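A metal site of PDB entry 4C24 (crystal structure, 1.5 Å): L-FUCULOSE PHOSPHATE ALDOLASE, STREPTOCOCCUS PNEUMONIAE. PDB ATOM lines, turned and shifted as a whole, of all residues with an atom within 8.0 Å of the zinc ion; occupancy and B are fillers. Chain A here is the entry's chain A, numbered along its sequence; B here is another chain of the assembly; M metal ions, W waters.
Water W1 lies within hydrogen-bond range of OE2 of Glu 79, O of Gly 30 and OH of Tyr 119 of chain B.
Tyr 119 of chain B touches the zinc ion. Five residues have an atom within 4 Å of the zinc ion: Gly 30, His 98, His 100, His 160 and Tyr 119 of chain B.
A ring nitrogen (NE2) of His 98 sits close to the backbone carbonyl oxygen (O) of Gly 30 (3.0 Å). N of His 98 sits at hydrogen-bond distance from O of Asn 32. The backbone carbonyl oxygen (O) of Ile 162 lies within hydrogen-bond range of a ring nitrogen (ND1) of His 98, at 2.8 Å. NE2 of His 100 lies close to O of Gly 30 (3.2 Å). The backbone carbonyl oxygen (O) of His 160 lies within hydrogen-bond range of a ring nitrogen (NE2) of His 118 of chain B (2.8 Å). O of Gly 30 sits at hydrogen-bond distance from ND2 of Asn 32 (3.2 Å).
The zinc ion is bound by NE2 of His 98 (2.0 Å), NE2 of His 100 (2.0 Å), NE2 of His 160 (2.0 Å) and water W1 (2.1 Å). The zinc ion has four donor atoms within binding distance. Slightly farther from the zinc ion lies O of Gly 30 (2.6 Å).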
ATOM      1  N   GLY A  28      -4.910  22.400  30.000  1.00  0.00           N
ATOM      2  CA  GLY A  28      -6.112  22.298  30.819  1.00  0.00           C
ATOM      3  C   GLY A  28      -7.230  23.273  30.519  1.00  0.00           C
ATOM      4  O   GLY A  28      -8.408  23.003  30.783  1.00  0.00           O
ATOM      5  N   THR A  29      -6.875  24.440  29.980  1.00  0.00           N
ATOM      6  CA  THR A  29      -7.871  25.491  29.764  1.00  0.00           C
ATOM      7  C   THR A  29      -8.927  25.011  28.774  1.00  0.00           C
ATOM      8  O   THR A  29      -8.598  24.445  27.721  1.00  0.00           O
ATOM      9  CB  THR A  29      -7.240  26.808  29.262  1.00  0.00           C
ATOM     10  OG1 THR A  29      -6.834  26.674  27.891  1.00  0.00           O
ATOM     11  CG2 THR A  29      -6.037  27.203  30.140  1.00  0.00           C
ATOM     12  N   GLY A  30     -10.188  25.195  29.145  1.00  0.00           N
ATOM     13  CA  GLY A  30     -11.312  24.778  28.330  1.00  0.00           C
ATOM     14  C   GLY A  30     -11.510  23.274  28.259  1.00  0.00           C
ATOM     15  O   GLY A  30     -12.427  22.822  27.569  1.00  0.00           O
ATOM     16  N   GLY A  31     -10.652  22.517  28.955  1.00  0.00           N
ATOM     17  CA  GLY A  31     -10.713  21.044  28.967  1.00  0.00           C
ATOM     18  C   GLY A  31     -11.530  20.551  30.140  1.00  0.00           C
ATOM     19  O   GLY A  31     -11.688  21.245  31.133  1.00  0.00           O
ATOM     20  N   ASN A  32     -12.071  19.351  30.011  1.00  0.00           N
ATOM     21  CA  ASN A  32     -12.975  18.831  31.072  1.00  0.00           C
ATOM     22  C   ASN A  32     -13.091  17.331  30.984  1.00  0.00           C
ATOM     23  O   ASN A  32     -12.877  16.736  29.929  1.00  0.00           O
ATOM     24  CB  ASN A  32     -14.353  19.538  31.112  1.00  0.00           C
ATOM     25  CG  ASN A  32     -14.749  20.122  29.778  1.00  0.00           C
ATOM     26  OD1 ASN A  32     -15.251  19.410  28.911  1.00  0.00           O
ATOM     27  ND2 ASN A  32     -14.507  21.422  29.595  1.00  0.00           N
ATOM     28  N   SER A  77     -18.187  22.410  34.810  1.00  0.00           N
ATOM     29  CA  SER A  77     -17.586  22.740  33.500  1.00  0.00           C
ATOM     30  C   SER A  77     -18.626  23.398  32.601  1.00  0.00           C
ATOM     31  O   SER A  77     -19.766  22.942  32.554  1.00  0.00           O
ATOM     32  CB  SER A  77     -17.132  21.475  32.821  1.00  0.00           C
ATOM     33  OG  SER A  77     -16.775  21.750  31.467  1.00  0.00           O
ATOM     34  N   SER A  78     -18.219  24.434  31.865  1.00  0.00           N
ATOM     35  CA  SER A  78     -19.148  25.069  30.906  1.00  0.00           C
ATOM     36  C   SER A  78     -19.622  24.056  29.862  1.00  0.00           C
ATOM     37  O   SER A  78     -20.674  24.275  29.245  1.00  0.00           O
ATOM     38  CB  SER A  78     -18.500  26.249  30.171  1.00  0.00           C
ATOM     39  OG  SER A  78     -17.335  25.856  29.502  1.00  0.00           O
ATOM     40  N   GLU A  79     -18.905  22.962  29.688  1.00  0.00           N
ATOM     41  CA  GLU A  79     -19.268  21.950  28.663  1.00  0.00           C
ATOM     42  C   GLU A  79     -20.092  20.777  29.206  1.00  0.00           C
ATOM     43  O   GLU A  79     -20.183  19.720  28.584  1.00  0.00           O
ATOM     44  CB  GLU A  79     -18.015  21.445  27.940  1.00  0.00           C
ATOM     45  CG  GLU A  79     -17.216  22.534  27.258  1.00  0.00           C
ATOM     46  CD  GLU A  79     -17.906  23.178  26.051  1.00  0.00           C
ATOM     47  OE1 GLU A  79     -19.104  22.936  25.760  1.00  0.00           O
ATOM     48  OE2 GLU A  79     -17.201  23.981  25.419  1.00  0.00           O
ATOM     49  N   MET A  82     -22.490  19.140  26.854  1.00  0.00           N
ATOM     50  CA  MET A  82     -21.842  18.362  25.802  1.00  0.00           C
ATOM     51  C   MET A  82     -21.498  16.965  26.288  1.00  0.00           C
ATOM     52  O   MET A  82     -21.637  15.983  25.588  1.00  0.00           O
ATOM     53  CB  MET A  82     -20.632  19.093  25.257  1.00  0.00           C
ATOM     54  CG  MET A  82     -19.828  18.274  24.288  1.00  0.00           C
ATOM     55  SD  MET A  82     -18.638  19.239  23.338  1.00  0.00           S
ATOM     56  CE  MET A  82     -17.561  19.749  24.686  1.00  0.00           C
ATOM     57  N   HIS A  98     -12.783  15.992  27.224  1.00  0.00           N
ATOM     58  CA  HIS A  98     -12.683  17.065  26.226  1.00  0.00           C
ATOM     59  C   HIS A  98     -11.373  17.799  26.455  1.00  0.00           C
ATOM     60  O   HIS A  98     -10.995  18.153  27.604  1.00  0.00           O
ATOM     61  CB  HIS A  98     -13.875  18.008  26.343  1.00  0.00           C
ATOM     62  CG  HIS A  98     -13.693  19.331  25.655  1.00  0.00           C
ATOM     63  ND1 HIS A  98     -13.563  19.449  24.294  1.00  0.00           N
ATOM     64  CD2 HIS A  98     -13.606  20.589  26.155  1.00  0.00           C
ATOM     65  CE1 HIS A  98     -13.405  20.720  23.976  1.00  0.00           C
ATOM     66  NE2 HIS A  98     -13.453  21.446  25.088  1.00  0.00           N
ATOM     67  N   ALA A  99     -10.637  18.035  25.368  1.00  0.00           N
ATOM     68  CA  ALA A  99      -9.364  18.680  25.470  1.00  0.00           C
ATOM     69  C   ALA A  99      -9.121  19.591  24.291  1.00  0.00           C
ATOM     70  O   ALA A  99      -9.709  19.369  23.238  1.00  0.00           O
ATOM     71  CB  ALA A  99      -8.249  17.643  25.559  1.00  0.00           C
ATOM     72  N   HIS A 100      -8.287  20.604  24.474  1.00  0.00           N
ATOM     73  CA  HIS A 100      -7.801  21.431  23.372  1.00  0.00           C
ATOM     74  C   HIS A 100      -6.383  20.968  23.115  1.00  0.00           C
ATOM     75  O   HIS A 100      -5.437  21.448  23.742  1.00  0.00           O
ATOM     76  CB  HIS A 100      -7.828  22.912  23.747  1.00  0.00           C
ATOM     77  CG  HIS A 100      -9.183  23.424  24.147  1.00  0.00           C
ATOM     78  ND1 HIS A 100      -9.455  24.757  24.280  1.00  0.00           N
ATOM     79  CD2 HIS A 100     -10.339  22.771  24.437  1.00  0.00           C
ATOM     80  CE1 HIS A 100     -10.715  24.911  24.687  1.00  0.00           C
ATOM     81  NE2 HIS A 100     -11.275  23.712  24.750  1.00  0.00           N
ATOM     82  N   TYR A 136     -18.750  27.670  22.307  1.00  0.00           N
ATOM     83  CA  TYR A 136     -18.433  26.817  23.442  1.00  0.00           C
ATOM     84  C   TYR A 136     -19.540  26.939  24.489  1.00  0.00           C
ATOM     85  O   TYR A 136     -20.165  28.000  24.647  1.00  0.00           O
ATOM     86  CB  TYR A 136     -17.065  27.196  24.030  1.00  0.00           C
ATOM     87  CG  TYR A 136     -17.094  28.308  25.035  1.00  0.00           C
ATOM     88  CD1 TYR A 136     -16.948  29.647  24.672  1.00  0.00           C
ATOM     89  CD2 TYR A 136     -17.260  28.016  26.397  1.00  0.00           C
ATOM     90  CE1 TYR A 136     -16.976  30.661  25.624  1.00  0.00           C
ATOM     91  CE2 TYR A 136     -17.309  29.009  27.348  1.00  0.00           C
ATOM     92  CZ  TYR A 136     -17.167  30.324  26.960  1.00  0.00           C
ATOM     93  OH  TYR A 136     -17.203  31.290  27.934  1.00  0.00           O
ATOM     94  N   GLY A 137     -19.799  25.817  25.153  1.00  0.00           N
ATOM     95  CA  GLY A 137     -20.701  25.794  26.292  1.00  0.00           C
ATOM     96  C   GLY A 137     -22.174  25.903  25.959  1.00  0.00           C
ATOM     97  O   GLY A 137     -22.998  26.088  26.844  1.00  0.00           O
ATOM     98  N   LEU A 141     -23.594  23.297  20.518  1.00  0.00           N
ATOM     99  CA  LEU A 141     -22.343  22.547  20.484  1.00  0.00           C
ATOM    100  C   LEU A 141     -22.560  21.121  20.979  1.00  0.00           C
ATOM    101  O   LEU A 141     -22.085  20.170  20.354  1.00  0.00           O
ATOM    102  CB  LEU A 141     -21.231  23.240  21.259  1.00  0.00           C
ATOM    103  CG  LEU A 141     -19.900  22.496  21.230  1.00  0.00           C
ATOM    104  CD1 LEU A 141     -19.381  22.322  19.805  1.00  0.00           C
ATOM    105  CD2 LEU A 141     -18.870  23.212  22.100  1.00  0.00           C
ATOM    106  N   LEU A 157     -14.188  19.187  17.372  1.00  0.00           N
ATOM    107  CA  LEU A 157     -15.109  20.298  17.572  1.00  0.00           C
ATOM    108  C   LEU A 157     -14.514  21.487  16.830  1.00  0.00           C
ATOM    109  O   LEU A 157     -13.418  21.952  17.129  1.00  0.00           O
ATOM    110  CB  LEU A 157     -15.204  20.630  19.057  1.00  0.00           C
ATOM    111  CG  LEU A 157     -15.600  19.428  19.921  1.00  0.00           C
ATOM    112  CD1 LEU A 157     -15.555  19.863  21.399  1.00  0.00           C
ATOM    113  CD2 LEU A 157     -16.946  18.815  19.538  1.00  0.00           C
ATOM    114  N   ASN A 159     -12.945  24.556  15.323  1.00  0.00           N
ATOM    115  CA  ASN A 159     -12.321  25.766  15.866  1.00  0.00           C
ATOM    116  C   ASN A 159     -12.192  25.702  17.372  1.00  0.00           C
ATOM    117  O   ASN A 159     -12.192  26.735  18.040  1.00  0.00           O
ATOM    118  CB  ASN A 159     -13.073  27.043  15.440  1.00  0.00           C
ATOM    119  CG  ASN A 159     -13.081  27.213  13.942  1.00  0.00           C
ATOM    120  OD1 ASN A 159     -12.132  27.709  13.348  1.00  0.00           O
ATOM    121  ND2 ASN A 159     -14.136  26.781  13.359  1.00  0.00           N
ATOM    122  N   HIS A 160     -12.061  24.482  17.880  1.00  0.00           N
ATOM    123  CA  HIS A 160     -12.182  24.285  19.337  1.00  0.00           C
ATOM    124  C   HIS A 160     -11.291  23.191  19.879  1.00  0.00           C
ATOM    125  O   HIS A 160     -10.338  23.497  20.612  1.00  0.00           O
ATOM    126  CB  HIS A 160     -13.651  24.030  19.666  1.00  0.00           C
ATOM    127  CG  HIS A 160     -13.943  23.984  21.130  1.00  0.00           C
ATOM    128  ND1 HIS A 160     -15.186  24.246  21.640  1.00  0.00           N
ATOM    129  CD2 HIS A 160     -13.144  23.696  22.194  1.00  0.00           C
ATOM    130  CE1 HIS A 160     -15.148  24.119  22.974  1.00  0.00           C
ATOM    131  NE2 HIS A 160     -13.916  23.785  23.319  1.00  0.00           N
ATOM    132  N   GLY A 161     -11.561  21.941  19.545  1.00  0.00           N
ATOM    133  CA  GLY A 161     -10.776  20.853  20.132  1.00  0.00           C
ATOM    134  C   GLY A 161     -11.322  19.493  19.842  1.00  0.00           C
ATOM    135  O   GLY A 161     -11.822  19.242  18.753  1.00  0.00           O
ATOM    136  N   ILE A 162     -11.247  18.599  20.811  1.00  0.00           N
ATOM    137  CA  ILE A 162     -11.607  17.224  20.615  1.00  0.00           C
ATOM    138  C   ILE A 162     -12.476  16.781  21.790  1.00  0.00           C
ATOM    139  O   ILE A 162     -12.352  17.312  22.895  1.00  0.00           O
ATOM    140  CB  ILE A 162     -10.341  16.336  20.516  1.00  0.00           C
ATOM    141  CG1 ILE A 162     -10.666  14.903  20.091  1.00  0.00           C
ATOM    142  CG2 ILE A 162      -9.572  16.322  21.845  1.00  0.00           C
ATOM    143  CD1 ILE A 162      -9.437  14.052  19.820  1.00  0.00           C
ATOM    144  N   HIS B 118      -8.994  30.084  16.218  1.00  0.00           N
ATOM    145  CA  HIS B 118      -9.451  29.422  17.424  1.00  0.00           C
ATOM    146  C   HIS B 118     -10.127  30.424  18.312  1.00  0.00           C
ATOM    147  O   HIS B 118      -9.629  31.554  18.466  1.00  0.00           O
ATOM    148  CB  HIS B 118      -8.273  28.800  18.155  1.00  0.00           C
ATOM    149  CG  HIS B 118      -8.702  27.807  19.188  1.00  0.00           C
ATOM    150  ND1 HIS B 118      -9.181  28.197  20.422  1.00  0.00           N
ATOM    151  CD2 HIS B 118      -8.769  26.454  19.154  1.00  0.00           C
ATOM    152  CE1 HIS B 118      -9.503  27.106  21.107  1.00  0.00           C
ATOM    153  NE2 HIS B 118      -9.272  26.045  20.363  1.00  0.00           N
ATOM    154  N   TYR B 119     -11.253  30.043  18.916  1.00  0.00           N
ATOM    155  CA  TYR B 119     -12.037  30.984  19.720  1.00  0.00           C
ATOM    156  C   TYR B 119     -11.317  31.535  20.954  1.00  0.00           C
ATOM    157  O   TYR B 119     -11.659  32.609  21.442  1.00  0.00           O
ATOM    158  CB  TYR B 119     -13.393  30.411  20.111  1.00  0.00           C
ATOM    159  CG  TYR B 119     -13.368  29.492  21.294  1.00  0.00           C
ATOM    160  CD1 TYR B 119     -13.521  30.010  22.560  1.00  0.00           C
ATOM    161  CD2 TYR B 119     -13.196  28.118  21.153  1.00  0.00           C
ATOM    162  CE1 TYR B 119     -13.500  29.207  23.675  1.00  0.00           C
ATOM    163  CE2 TYR B 119     -13.180  27.292  22.274  1.00  0.00           C
ATOM    164  CZ  TYR B 119     -13.338  27.856  23.530  1.00  0.00           C
ATOM    165  OH  TYR B 119     -13.303  27.039  24.640  1.00  0.00           O
ATOM    166  N   MET B 120     -10.309  30.816  21.439  1.00  0.00           N
ATOM    167  CA  MET B 120      -9.620  31.230  22.670  1.00  0.00           C
ATOM    168  C   MET B 120      -8.833  32.516  22.536  1.00  0.00           C
ATOM    169  O   MET B 120      -8.389  33.114  23.526  1.00  0.00           O
ATOM    170  CB  MET B 120      -8.731  30.111  23.197  1.00  0.00           C
ATOM    171  CG  MET B 120      -9.514  29.021  23.886  1.00  0.00           C
ATOM    172  SD  MET B 120     -10.400  29.577  25.358  1.00  0.00           S
ATOM    173  CE  MET B 120      -9.118  30.410  26.253  1.00  0.00           C
HETATM  174 ZN    ZN M   1     -13.202  23.414  25.156  1.00  0.00          ZN
HETATM  175  O   HOH W   1     -14.540  24.524  26.324  1.00  0.00           O
